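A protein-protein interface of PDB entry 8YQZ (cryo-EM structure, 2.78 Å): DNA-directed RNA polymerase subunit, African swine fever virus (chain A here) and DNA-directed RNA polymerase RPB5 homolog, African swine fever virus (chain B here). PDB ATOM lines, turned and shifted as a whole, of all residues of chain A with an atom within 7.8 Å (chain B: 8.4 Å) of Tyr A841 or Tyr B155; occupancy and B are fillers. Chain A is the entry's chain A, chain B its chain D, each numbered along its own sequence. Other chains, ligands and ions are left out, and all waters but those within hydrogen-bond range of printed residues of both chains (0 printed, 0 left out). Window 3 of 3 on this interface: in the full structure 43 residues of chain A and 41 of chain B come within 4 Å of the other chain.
The backbone carbonyl oxygen of Arg B153 sits at hydrogen-bond distance from the side-chain hydroxyl of Tyr A841 (3.3 Å). The guanidinium group (NH1) of Arg A843 is in salt-bridge range of the side-chain carboxylate (OE1) of Glu B154, at 3.0 Å. O of Asp B160 lies within hydrogen-bond range of N of Leu A850, at 2.8 Å. OH of Tyr A990 is in hydrogen-bond range of OE2 of Glu B154.
Of the 12 printed residues of chain B, 6 touch a printed residue of chain A. Printed residues of chain B that touch a printed residue of chain A: Phe B150, Arg B153, Glu B154, Tyr B155, Leu B156 and Asp B160. Hydrophobic or aromatic side chains of chain B that line the printed part of chain A: Phe B150, Tyr B155 and Leu B156. Of the 21 printed residues of chain A, 7 touch a printed residue of chain B. Hydrophobic or aromatic side chains of chain A that line the printed part of chain B: Tyr A841, Leu A850, Pro A988 and Tyr A990. Among the printed residues, 13 pairs touch across the chains.
Printed residues of chain B within 4 Å of Tyr A841: Arg B153 (3.3 Å), Glu B154 (3.7 Å) and Tyr B155 (3.5 Å). Tyr B155 touches one residue of chain A. Printed residues of chain A within 4 Å of Phe B150: Gln A853. Printed residues of chain B within 4 Å of Arg A843: Glu B154 and Leu B156. Of the printed residues of chain A, Glu B154 touches Tyr A841 (3.7 Å), Arg A843 (3.0 Å), Gln A853 (3.5 Å) and Tyr A990 (3.0 Å). Of the printed residues of chain B, Gln A853 touches Phe B150 and Glu B154. Of the printed residues of chain A, Asp B160 touches Thr A848 (3.5 Å) and Leu A850 (2.8 Å). Tyr A1426 touches none of the printed residues of chain B. The nearest residue of chain A that does not touch Tyr B155 is Arg A843 (5.4 Å). The nearest printed residue of chain A that does not touch Arg B153 is Leu A991 (4.5 Å).
OH of Tyr A841 touches O of Glu B154, 3.7 Å away. CD2 of Tyr B155 touches OH of Tyr A841, at 3.5 Å. Arg A843 touches Leu B156. Thr A848 touches Asp B160 (CB to OD2, 3.5 Å). Leu B156 touches Leu A850. Gln A853 touches Phe B150 (NE2 to CZ, 3.3 Å). Glu B154 touches Gln A853 (OE1 to OE1, 3.5 Å). Arg B153 touches Pro A988. Arg B153 touches Tyr A990 (NH1 to OH, 3.5 Å).
The guanidinium group of Arg A843 lies within salt-bridge range of the side-chain carboxylate of Asp A839, 3.3 Å away. The backbone carbonyl oxygen (O) of Leu B151 lies within hydrogen-bond range of the backbone NH (N) of Leu B156, at 3.1 Å. OE2 of Glu B154 lies within salt-bridge range of NH1 of Arg B153, at 2.7 Å. The side-chain carboxylate of Asp B160 sits at hydrogen-bond distance from the backbone NH of Gln B157 (3.3 Å).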
ATOM      1  N   VAL A 838     -18.028  -1.974 -25.972  1.00  0.00           N
ATOM      2  CA  VAL A 838     -19.195  -2.828 -25.766  1.00  0.00           C
ATOM      3  C   VAL A 838     -19.839  -2.516 -24.417  1.00  0.00           C
ATOM      4  O   VAL A 838     -19.155  -2.440 -23.394  1.00  0.00           O
ATOM      5  CB  VAL A 838     -18.803  -4.311 -25.872  1.00  0.00           C
ATOM      6  CG1 VAL A 838     -19.981  -5.217 -25.591  1.00  0.00           C
ATOM      7  CG2 VAL A 838     -18.259  -4.607 -27.234  1.00  0.00           C
ATOM      8  N   ASP A 839     -21.162  -2.348 -24.417  1.00  0.00           N
ATOM      9  CA  ASP A 839     -21.961  -2.007 -23.244  1.00  0.00           C
ATOM     10  C   ASP A 839     -22.300  -3.238 -22.418  1.00  0.00           C
ATOM     11  O   ASP A 839     -21.805  -4.336 -22.659  1.00  0.00           O
ATOM     12  CB  ASP A 839     -23.279  -1.362 -23.654  1.00  0.00           C
ATOM     13  CG  ASP A 839     -23.105  -0.021 -24.221  1.00  0.00           C
ATOM     14  OD1 ASP A 839     -22.006   0.539 -24.076  1.00  0.00           O
ATOM     15  OD2 ASP A 839     -24.071   0.489 -24.804  1.00  0.00           O
ATOM     16  N   TYR A 840     -23.207  -3.057 -21.458  1.00  0.00           N
ATOM     17  CA  TYR A 840     -23.824  -4.146 -20.714  1.00  0.00           C
ATOM     18  C   TYR A 840     -25.002  -4.762 -21.441  1.00  0.00           C
ATOM     19  O   TYR A 840     -25.588  -5.721 -20.940  1.00  0.00           O
ATOM     20  CB  TYR A 840     -24.291  -3.658 -19.349  1.00  0.00           C
ATOM     21  CG  TYR A 840     -23.169  -3.509 -18.373  1.00  0.00           C
ATOM     22  CD1 TYR A 840     -22.368  -4.577 -18.050  1.00  0.00           C
ATOM     23  CD2 TYR A 840     -22.902  -2.290 -17.786  1.00  0.00           C
ATOM     24  CE1 TYR A 840     -21.340  -4.437 -17.175  1.00  0.00           C
ATOM     25  CE2 TYR A 840     -21.873  -2.142 -16.913  1.00  0.00           C
ATOM     26  CZ  TYR A 840     -21.095  -3.217 -16.606  1.00  0.00           C
ATOM     27  OH  TYR A 840     -20.066  -3.067 -15.724  1.00  0.00           O
ATOM     28  N   TYR A 841     -25.394  -4.211 -22.578  1.00  0.00           N
ATOM     29  CA  TYR A 841     -26.422  -4.794 -23.419  1.00  0.00           C
ATOM     30  C   TYR A 841     -25.844  -5.477 -24.641  1.00  0.00           C
ATOM     31  O   TYR A 841     -26.605  -5.999 -25.453  1.00  0.00           O
ATOM     32  CB  TYR A 841     -27.412  -3.723 -23.864  1.00  0.00           C
ATOM     33  CG  TYR A 841     -28.338  -3.222 -22.795  1.00  0.00           C
ATOM     34  CD1 TYR A 841     -27.906  -2.317 -21.849  1.00  0.00           C
ATOM     35  CD2 TYR A 841     -29.659  -3.618 -22.761  1.00  0.00           C
ATOM     36  CE1 TYR A 841     -28.749  -1.848 -20.882  1.00  0.00           C
ATOM     37  CE2 TYR A 841     -30.510  -3.150 -21.797  1.00  0.00           C
ATOM     38  CZ  TYR A 841     -30.050  -2.266 -20.864  1.00  0.00           C
ATOM     39  OH  TYR A 841     -30.901  -1.801 -19.903  1.00  0.00           O
ATOM     40  N   ARG A 842     -24.519  -5.490 -24.774  1.00  0.00           N
ATOM     41  CA  ARG A 842     -23.766  -5.883 -25.959  1.00  0.00           C
ATOM     42  C   ARG A 842     -23.916  -4.900 -27.107  1.00  0.00           C
ATOM     43  O   ARG A 842     -23.553  -5.224 -28.234  1.00  0.00           O
ATOM     44  CB  ARG A 842     -24.126  -7.289 -26.447  1.00  0.00           C
ATOM     45  CG  ARG A 842     -23.176  -8.386 -26.052  1.00  0.00           C
ATOM     46  CD  ARG A 842     -23.376  -8.713 -24.632  1.00  0.00           C
ATOM     47  NE  ARG A 842     -22.641  -9.887 -24.189  1.00  0.00           N
ATOM     48  CZ  ARG A 842     -23.179 -10.898 -23.525  1.00  0.00           C
ATOM     49  NH1 ARG A 842     -24.480 -10.985 -23.331  1.00  0.00           N
ATOM     50  NH2 ARG A 842     -22.386 -11.824 -23.010  1.00  0.00           N
ATOM     51  N   ARG A 843     -24.437  -3.707 -26.857  1.00  0.00           N
ATOM     52  CA  ARG A 843     -24.424  -2.658 -27.861  1.00  0.00           C
ATOM     53  C   ARG A 843     -23.044  -2.023 -27.925  1.00  0.00           C
ATOM     54  O   ARG A 843     -22.211  -2.201 -27.043  1.00  0.00           O
ATOM     55  CB  ARG A 843     -25.452  -1.579 -27.534  1.00  0.00           C
ATOM     56  CG  ARG A 843     -26.787  -2.085 -27.081  1.00  0.00           C
ATOM     57  CD  ARG A 843     -27.716  -0.947 -26.819  1.00  0.00           C
ATOM     58  NE  ARG A 843     -27.175  -0.030 -25.829  1.00  0.00           N
ATOM     59  CZ  ARG A 843     -27.780   0.319 -24.707  1.00  0.00           C
ATOM     60  NH1 ARG A 843     -28.985  -0.114 -24.411  1.00  0.00           N
ATOM     61  NH2 ARG A 843     -27.154   1.122 -23.862  1.00  0.00           N
ATOM     62  N   VAL A 844     -22.809  -1.260 -28.978  1.00  0.00           N
ATOM     63  CA  VAL A 844     -21.594  -0.471 -29.121  1.00  0.00           C
ATOM     64  C   VAL A 844     -21.993   0.994 -29.119  1.00  0.00           C
ATOM     65  O   VAL A 844     -22.865   1.404 -29.885  1.00  0.00           O
ATOM     66  CB  VAL A 844     -20.829  -0.834 -30.402  1.00  0.00           C
ATOM     67  CG1 VAL A 844     -19.567  -0.039 -30.492  1.00  0.00           C
ATOM     68  CG2 VAL A 844     -20.533  -2.303 -30.427  1.00  0.00           C
ATOM     69  N   THR A 848     -22.488   7.327 -24.759  1.00  0.00           N
ATOM     70  CA  THR A 848     -23.882   6.985 -24.522  1.00  0.00           C
ATOM     71  C   THR A 848     -24.541   6.702 -25.853  1.00  0.00           C
ATOM     72  O   THR A 848     -25.561   6.018 -25.929  1.00  0.00           O
ATOM     73  CB  THR A 848     -24.620   8.090 -23.769  1.00  0.00           C
ATOM     74  OG1 THR A 848     -23.912   9.327 -23.908  1.00  0.00           O
ATOM     75  CG2 THR A 848     -24.764   7.728 -22.303  1.00  0.00           C
ATOM     76  N   LEU A 850     -25.405   5.393 -29.348  1.00  0.00           N
ATOM     77  CA  LEU A 850     -25.328   4.095 -29.994  1.00  0.00           C
ATOM     78  C   LEU A 850     -24.594   4.171 -31.321  1.00  0.00           C
ATOM     79  O   LEU A 850     -24.879   5.033 -32.150  1.00  0.00           O
ATOM     80  CB  LEU A 850     -26.730   3.550 -30.221  1.00  0.00           C
ATOM     81  CG  LEU A 850     -27.213   2.448 -29.301  1.00  0.00           C
ATOM     82  CD1 LEU A 850     -27.041   2.888 -27.875  1.00  0.00           C
ATOM     83  CD2 LEU A 850     -28.646   2.140 -29.605  1.00  0.00           C
ATOM     84  N   GLN A 852     -23.776   0.710 -32.700  1.00  0.00           N
ATOM     85  CA  GLN A 852     -24.412  -0.525 -33.129  1.00  0.00           C
ATOM     86  C   GLN A 852     -25.408  -0.940 -32.067  1.00  0.00           C
ATOM     87  O   GLN A 852     -25.171  -0.733 -30.881  1.00  0.00           O
ATOM     88  CB  GLN A 852     -23.398  -1.638 -33.344  1.00  0.00           C
ATOM     89  CG  GLN A 852     -22.514  -1.408 -34.523  1.00  0.00           C
ATOM     90  CD  GLN A 852     -21.605  -2.554 -34.789  1.00  0.00           C
ATOM     91  OE1 GLN A 852     -21.463  -3.438 -33.970  1.00  0.00           O
ATOM     92  NE2 GLN A 852     -20.997  -2.561 -35.951  1.00  0.00           N
ATOM     93  N   GLN A 853     -26.535  -1.506 -32.494  1.00  0.00           N
ATOM     94  CA  GLN A 853     -27.508  -2.018 -31.540  1.00  0.00           C
ATOM     95  C   GLN A 853     -27.063  -3.344 -30.936  1.00  0.00           C
ATOM     96  O   GLN A 853     -27.445  -3.671 -29.813  1.00  0.00           O
ATOM     97  CB  GLN A 853     -28.872  -2.146 -32.214  1.00  0.00           C
ATOM     98  CG  GLN A 853     -29.926  -2.808 -31.372  1.00  0.00           C
ATOM     99  CD  GLN A 853     -30.552  -1.880 -30.370  1.00  0.00           C
ATOM    100  OE1 GLN A 853     -30.265  -1.941 -29.181  1.00  0.00           O
ATOM    101  NE2 GLN A 853     -31.428  -1.016 -30.845  1.00  0.00           N
ATOM    102  N   LEU A 854     -26.268  -4.114 -31.659  1.00  0.00           N
ATOM    103  CA  LEU A 854     -25.662  -5.339 -31.167  1.00  0.00           C
ATOM    104  C   LEU A 854     -24.348  -5.519 -31.896  1.00  0.00           C
ATOM    105  O   LEU A 854     -24.306  -5.404 -33.117  1.00  0.00           O
ATOM    106  CB  LEU A 854     -26.568  -6.546 -31.398  1.00  0.00           C
ATOM    107  CG  LEU A 854     -26.227  -7.881 -30.746  1.00  0.00           C
ATOM    108  CD1 LEU A 854     -26.334  -7.818 -29.244  1.00  0.00           C
ATOM    109  CD2 LEU A 854     -27.144  -8.929 -31.280  1.00  0.00           C
ATOM    110  N   TYR A 855     -23.283  -5.794 -31.157  1.00  0.00           N
ATOM    111  CA  TYR A 855     -21.962  -5.883 -31.764  1.00  0.00           C
ATOM    112  C   TYR A 855     -21.940  -6.954 -32.842  1.00  0.00           C
ATOM    113  O   TYR A 855     -22.318  -8.099 -32.596  1.00  0.00           O
ATOM    114  CB  TYR A 855     -20.907  -6.182 -30.703  1.00  0.00           C
ATOM    115  CG  TYR A 855     -19.553  -6.463 -31.292  1.00  0.00           C
ATOM    116  CD1 TYR A 855     -18.851  -5.472 -31.947  1.00  0.00           C
ATOM    117  CD2 TYR A 855     -18.985  -7.717 -31.217  1.00  0.00           C
ATOM    118  CE1 TYR A 855     -17.640  -5.717 -32.497  1.00  0.00           C
ATOM    119  CE2 TYR A 855     -17.769  -7.962 -31.764  1.00  0.00           C
ATOM    120  CZ  TYR A 855     -17.101  -6.959 -32.404  1.00  0.00           C
ATOM    121  OH  TYR A 855     -15.869  -7.188 -32.953  1.00  0.00           O
ATOM    122  N   GLY A 859     -23.454 -10.323 -31.829  1.00  0.00           N
ATOM    123  CA  GLY A 859     -22.965 -10.286 -30.468  1.00  0.00           C
ATOM    124  C   GLY A 859     -21.894 -11.287 -30.121  1.00  0.00           C
ATOM    125  O   GLY A 859     -21.802 -11.689 -28.965  1.00  0.00           O
ATOM    126  N   PHE A 975     -28.816 -14.209 -24.662  1.00  0.00           N
ATOM    127  CA  PHE A 975     -28.412 -12.815 -24.679  1.00  0.00           C
ATOM    128  C   PHE A 975     -28.891 -12.041 -23.465  1.00  0.00           C
ATOM    129  O   PHE A 975     -28.565 -10.859 -23.356  1.00  0.00           O
ATOM    130  CB  PHE A 975     -28.940 -12.127 -25.935  1.00  0.00           C
ATOM    131  CG  PHE A 975     -28.348 -12.638 -27.201  1.00  0.00           C
ATOM    132  CD1 PHE A 975     -27.055 -12.322 -27.551  1.00  0.00           C
ATOM    133  CD2 PHE A 975     -29.089 -13.428 -28.053  1.00  0.00           C
ATOM    134  CE1 PHE A 975     -26.519 -12.794 -28.713  1.00  0.00           C
ATOM    135  CE2 PHE A 975     -28.551 -13.897 -29.214  1.00  0.00           C
ATOM    136  CZ  PHE A 975     -27.269 -13.580 -29.543  1.00  0.00           C
ATOM    137  N   PRO A 988     -36.786  -8.506 -26.754  1.00  0.00           N
ATOM    138  CA  PRO A 988     -36.741  -7.479 -27.794  1.00  0.00           C
ATOM    139  C   PRO A 988     -36.603  -8.090 -29.180  1.00  0.00           C
ATOM    140  O   PRO A 988     -36.038  -9.167 -29.354  1.00  0.00           O
ATOM    141  CB  PRO A 988     -35.508  -6.655 -27.421  1.00  0.00           C
ATOM    142  CG  PRO A 988     -35.280  -6.931 -26.019  1.00  0.00           C
ATOM    143  CD  PRO A 988     -35.725  -8.314 -25.757  1.00  0.00           C
ATOM    144  N   TYR A 990     -34.860  -7.126 -31.740  1.00  0.00           N
ATOM    145  CA  TYR A 990     -33.499  -7.203 -32.252  1.00  0.00           C
ATOM    146  C   TYR A 990     -32.723  -8.377 -31.670  1.00  0.00           C
ATOM    147  O   TYR A 990     -31.683  -8.739 -32.219  1.00  0.00           O
ATOM    148  CB  TYR A 990     -32.758  -5.887 -31.999  1.00  0.00           C
ATOM    149  CG  TYR A 990     -32.266  -5.684 -30.586  1.00  0.00           C
ATOM    150  CD1 TYR A 990     -33.095  -5.173 -29.609  1.00  0.00           C
ATOM    151  CD2 TYR A 990     -30.967  -6.005 -30.232  1.00  0.00           C
ATOM    152  CE1 TYR A 990     -32.650  -4.990 -28.334  1.00  0.00           C
ATOM    153  CE2 TYR A 990     -30.522  -5.833 -28.953  1.00  0.00           C
ATOM    154  CZ  TYR A 990     -31.367  -5.324 -28.008  1.00  0.00           C
ATOM    155  OH  TYR A 990     -30.928  -5.139 -26.723  1.00  0.00           O
ATOM    156  N   LEU A 991     -33.200  -8.977 -30.581  1.00  0.00           N
ATOM    157  CA  LEU A 991     -32.556 -10.169 -30.041  1.00  0.00           C
ATOM    158  C   LEU A 991     -33.182 -11.446 -30.580  1.00  0.00           C
ATOM    159  O   LEU A 991     -32.542 -12.497 -30.563  1.00  0.00           O
ATOM    160  CB  LEU A 991     -32.616 -10.169 -28.516  1.00  0.00           C
ATOM    161  CG  LEU A 991     -31.718  -9.202 -27.755  1.00  0.00           C
ATOM    162  CD1 LEU A 991     -31.885  -9.403 -26.277  1.00  0.00           C
ATOM    163  CD2 LEU A 991     -30.271  -9.365 -28.157  1.00  0.00           C
ATOM    164  N   ILE A1035     -19.500 -11.657 -26.898  1.00  0.00           N
ATOM    165  CA  ILE A1035     -18.485 -10.632 -26.683  1.00  0.00           C
ATOM    166  C   ILE A1035     -18.586 -10.086 -25.257  1.00  0.00           C
ATOM    167  O   ILE A1035     -19.671  -9.984 -24.680  1.00  0.00           O
ATOM    168  CB  ILE A1035     -18.624  -9.523 -27.747  1.00  0.00           C
ATOM    169  CG1 ILE A1035     -17.425  -8.581 -27.750  1.00  0.00           C
ATOM    170  CG2 ILE A1035     -19.892  -8.737 -27.572  1.00  0.00           C
ATOM    171  CD1 ILE A1035     -16.250  -9.083 -28.482  1.00  0.00           C
ATOM    172  N   TYR A1037     -18.430  -7.536 -22.038  1.00  0.00           N
ATOM    173  CA  TYR A1037     -18.724  -6.152 -21.707  1.00  0.00           C
ATOM    174  C   TYR A1037     -17.429  -5.379 -21.526  1.00  0.00           C
ATOM    175  O   TYR A1037     -16.522  -5.829 -20.826  1.00  0.00           O
ATOM    176  CB  TYR A1037     -19.525  -6.075 -20.415  1.00  0.00           C
ATOM    177  CG  TYR A1037     -20.770  -6.913 -20.321  1.00  0.00           C
ATOM    178  CD1 TYR A1037     -21.705  -6.941 -21.333  1.00  0.00           C
ATOM    179  CD2 TYR A1037     -21.002  -7.685 -19.201  1.00  0.00           C
ATOM    180  CE1 TYR A1037     -22.838  -7.696 -21.218  1.00  0.00           C
ATOM    181  CE2 TYR A1037     -22.124  -8.446 -19.089  1.00  0.00           C
ATOM    182  CZ  TYR A1037     -23.037  -8.444 -20.095  1.00  0.00           C
ATOM    183  OH  TYR A1037     -24.160  -9.208 -19.973  1.00  0.00           O
ATOM    184  N   TYR A1426     -13.736  -2.280 -16.362  1.00  0.00           N
ATOM    185  CA  TYR A1426     -15.044  -1.824 -16.798  1.00  0.00           C
ATOM    186  C   TYR A1426     -16.076  -1.912 -15.685  1.00  0.00           C
ATOM    187  O   TYR A1426     -16.944  -1.045 -15.572  1.00  0.00           O
ATOM    188  CB  TYR A1426     -15.491  -2.628 -18.012  1.00  0.00           C
ATOM    189  CG  TYR A1426     -16.708  -2.071 -18.682  1.00  0.00           C
ATOM    190  CD1 TYR A1426     -16.663  -0.865 -19.343  1.00  0.00           C
ATOM    191  CD2 TYR A1426     -17.907  -2.746 -18.640  1.00  0.00           C
ATOM    192  CE1 TYR A1426     -17.771  -0.356 -19.938  1.00  0.00           C
ATOM    193  CE2 TYR A1426     -19.019  -2.240 -19.239  1.00  0.00           C
ATOM    194  CZ  TYR A1426     -18.947  -1.045 -19.883  1.00  0.00           C
ATOM    195  OH  TYR A1426     -20.052  -0.523 -20.484  1.00  0.00           O
ATOM    196  N   GLN B 148     -41.344   4.331 -26.742  1.00  0.00           N
ATOM    197  CA  GLN B 148     -41.165   4.582 -25.322  1.00  0.00           C
ATOM    198  C   GLN B 148     -40.883   3.298 -24.566  1.00  0.00           C
ATOM    199  O   GLN B 148     -40.019   3.265 -23.688  1.00  0.00           O
ATOM    200  CB  GLN B 148     -42.400   5.275 -24.763  1.00  0.00           C
ATOM    201  CG  GLN B 148     -42.086   6.446 -23.866  1.00  0.00           C
ATOM    202  CD  GLN B 148     -41.050   7.369 -24.463  1.00  0.00           C
ATOM    203  OE1 GLN B 148     -41.247   7.929 -25.540  1.00  0.00           O
ATOM    204  NE2 GLN B 148     -39.933   7.534 -23.765  1.00  0.00           N
ATOM    205  N   GLU B 149     -41.604   2.229 -24.885  1.00  0.00           N
ATOM    206  CA  GLU B 149     -41.362   0.972 -24.192  1.00  0.00           C
ATOM    207  C   GLU B 149     -39.974   0.425 -24.509  1.00  0.00           C
ATOM    208  O   GLU B 149     -39.280  -0.085 -23.617  1.00  0.00           O
ATOM    209  CB  GLU B 149     -42.462  -0.026 -24.543  1.00  0.00           C
ATOM    210  CG  GLU B 149     -42.069  -1.474 -24.424  1.00  0.00           C
ATOM    211  CD  GLU B 149     -42.927  -2.380 -25.281  1.00  0.00           C
ATOM    212  OE1 GLU B 149     -43.053  -2.119 -26.495  1.00  0.00           O
ATOM    213  OE2 GLU B 149     -43.482  -3.355 -24.734  1.00  0.00           O
ATOM    214  N   PHE B 150     -39.540   0.548 -25.767  1.00  0.00           N
ATOM    215  CA  PHE B 150     -38.194   0.133 -26.145  1.00  0.00           C
ATOM    216  C   PHE B 150     -37.135   0.916 -25.376  1.00  0.00           C
ATOM    217  O   PHE B 150     -36.234   0.332 -24.767  1.00  0.00           O
ATOM    218  CB  PHE B 150     -38.015   0.306 -27.656  1.00  0.00           C
ATOM    219  CG  PHE B 150     -36.600   0.153 -28.129  1.00  0.00           C
ATOM    220  CD1 PHE B 150     -36.039  -1.093 -28.282  1.00  0.00           C
ATOM    221  CD2 PHE B 150     -35.835   1.259 -28.434  1.00  0.00           C
ATOM    222  CE1 PHE B 150     -34.748  -1.223 -28.710  1.00  0.00           C
ATOM    223  CE2 PHE B 150     -34.549   1.123 -28.863  1.00  0.00           C
ATOM    224  CZ  PHE B 150     -34.006  -0.113 -29.002  1.00  0.00           C
ATOM    225  N   LEU B 151     -37.249   2.245 -25.366  1.00  0.00           N
ATOM    226  CA  LEU B 151     -36.258   3.072 -24.688  1.00  0.00           C
ATOM    227  C   LEU B 151     -36.273   2.848 -23.184  1.00  0.00           C
ATOM    228  O   LEU B 151     -35.236   2.957 -22.528  1.00  0.00           O
ATOM    229  CB  LEU B 151     -36.497   4.544 -24.998  1.00  0.00           C
ATOM    230  CG  LEU B 151     -36.350   5.025 -26.435  1.00  0.00           C
ATOM    231  CD1 LEU B 151     -36.901   6.419 -26.556  1.00  0.00           C
ATOM    232  CD2 LEU B 151     -34.918   4.978 -26.886  1.00  0.00           C
ATOM    233  N   GLY B 152     -37.440   2.567 -22.615  1.00  0.00           N
ATOM    234  CA  GLY B 152     -37.505   2.283 -21.197  1.00  0.00           C
ATOM    235  C   GLY B 152     -36.838   0.976 -20.827  1.00  0.00           C
ATOM    236  O   GLY B 152     -36.165   0.885 -19.799  1.00  0.00           O
ATOM    237  N   ARG B 153     -37.024  -0.057 -21.644  1.00  0.00           N
ATOM    238  CA  ARG B 153     -36.307  -1.302 -21.393  1.00  0.00           C
ATOM    239  C   ARG B 153     -34.806  -1.124 -21.580  1.00  0.00           C
ATOM    240  O   ARG B 153     -34.013  -1.763 -20.889  1.00  0.00           O
ATOM    241  CB  ARG B 153     -36.838  -2.404 -22.302  1.00  0.00           C
ATOM    242  CG  ARG B 153     -36.364  -3.793 -21.961  1.00  0.00           C
ATOM    243  CD  ARG B 153     -35.317  -4.278 -22.930  1.00  0.00           C
ATOM    244  NE  ARG B 153     -34.775  -5.571 -22.536  1.00  0.00           N
ATOM    245  CZ  ARG B 153     -33.603  -6.042 -22.933  1.00  0.00           C
ATOM    246  NH1 ARG B 153     -32.820  -5.354 -23.739  1.00  0.00           N
ATOM    247  NH2 ARG B 153     -33.211  -7.237 -22.514  1.00  0.00           N
ATOM    248  N   GLU B 154     -34.398  -0.265 -22.504  1.00  0.00           N
ATOM    249  CA  GLU B 154     -32.995  -0.111 -22.848  1.00  0.00           C
ATOM    250  C   GLU B 154     -32.283   0.971 -22.051  1.00  0.00           C
ATOM    251  O   GLU B 154     -31.070   1.117 -22.204  1.00  0.00           O
ATOM    252  CB  GLU B 154     -32.863   0.198 -24.337  1.00  0.00           C
ATOM    253  CG  GLU B 154     -33.374  -0.898 -25.226  1.00  0.00           C
ATOM    254  CD  GLU B 154     -32.352  -1.967 -25.491  1.00  0.00           C
ATOM    255  OE1 GLU B 154     -31.197  -1.633 -25.817  1.00  0.00           O
ATOM    256  OE2 GLU B 154     -32.709  -3.152 -25.371  1.00  0.00           O
ATOM    257  N   TYR B 155     -32.996   1.724 -21.217  1.00  0.00           N
ATOM    258  CA  TYR B 155     -32.426   2.820 -20.428  1.00  0.00           C
ATOM    259  C   TYR B 155     -31.740   3.852 -21.320  1.00  0.00           C
ATOM    260  O   TYR B 155     -30.593   4.234 -21.101  1.00  0.00           O
ATOM    261  CB  TYR B 155     -31.455   2.297 -19.370  1.00  0.00           C
ATOM    262  CG  TYR B 155     -32.100   1.887 -18.077  1.00  0.00           C
ATOM    263  CD1 TYR B 155     -32.526   2.832 -17.166  1.00  0.00           C
ATOM    264  CD2 TYR B 155     -32.274   0.560 -17.760  1.00  0.00           C
ATOM    265  CE1 TYR B 155     -33.115   2.463 -15.985  1.00  0.00           C
ATOM    266  CE2 TYR B 155     -32.859   0.184 -16.580  1.00  0.00           C
ATOM    267  CZ  TYR B 155     -33.277   1.139 -15.697  1.00  0.00           C
ATOM    268  OH  TYR B 155     -33.863   0.756 -14.521  1.00  0.00           O
ATOM    269  N   LEU B 156     -32.465   4.316 -22.331  1.00  0.00           N
ATOM    270  CA  LEU B 156     -31.939   5.228 -23.331  1.00  0.00           C
ATOM    271  C   LEU B 156     -32.832   6.451 -23.454  1.00  0.00           C
ATOM    272  O   LEU B 156     -34.013   6.421 -23.104  1.00  0.00           O
ATOM    273  CB  LEU B 156     -31.829   4.548 -24.697  1.00  0.00           C
ATOM    274  CG  LEU B 156     -30.704   3.550 -24.955  1.00  0.00           C
ATOM    275  CD1 LEU B 156     -30.939   2.844 -26.262  1.00  0.00           C
ATOM    276  CD2 LEU B 156     -29.374   4.236 -24.976  1.00  0.00           C
ATOM    277  N   GLN B 157     -32.268   7.494 -23.922  1.00  0.00           N
ATOM    278  CA  GLN B 157     -32.903   8.719 -24.365  1.00  0.00           C
ATOM    279  C   GLN B 157     -32.998   8.737 -25.884  1.00  0.00           C
ATOM    280  O   GLN B 157     -32.207   8.084 -26.562  1.00  0.00           O
ATOM    281  CB  GLN B 157     -32.119   9.946 -23.892  1.00  0.00           C
ATOM    282  CG  GLN B 157     -31.926  10.037 -22.392  1.00  0.00           C
ATOM    283  CD  GLN B 157     -33.219   9.892 -21.631  1.00  0.00           C
ATOM    284  OE1 GLN B 157     -34.242  10.451 -22.010  1.00  0.00           O
ATOM    285  NE2 GLN B 157     -33.186   9.122 -20.555  1.00  0.00           N
ATOM    286  N   PRO B 158     -33.956   9.463 -26.461  1.00  0.00           N
ATOM    287  CA  PRO B 158     -34.029   9.534 -27.927  1.00  0.00           C
ATOM    288  C   PRO B 158     -32.789  10.117 -28.564  1.00  0.00           C
ATOM    289  O   PRO B 158     -32.535   9.862 -29.743  1.00  0.00           O
ATOM    290  CB  PRO B 158     -35.254  10.419 -28.169  1.00  0.00           C
ATOM    291  CG  PRO B 158     -36.072  10.247 -26.959  1.00  0.00           C
ATOM    292  CD  PRO B 158     -35.122  10.095 -25.828  1.00  0.00           C
ATOM    293  N   ASP B 160     -29.757   9.339 -27.796  1.00  0.00           N
ATOM    294  CA  ASP B 160     -28.710   8.331 -27.840  1.00  0.00           C
ATOM    295  C   ASP B 160     -28.751   7.489 -29.105  1.00  0.00           C
ATOM    296  O   ASP B 160     -27.726   6.921 -29.483  1.00  0.00           O
ATOM    297  CB  ASP B 160     -28.820   7.414 -26.626  1.00  0.00           C
ATOM    298  CG  ASP B 160     -28.428   8.101 -25.343  1.00  0.00           C
ATOM    299  OD1 ASP B 160     -28.954   7.728 -24.279  1.00  0.00           O
ATOM    300  OD2 ASP B 160     -27.589   9.020 -25.394  1.00  0.00           O
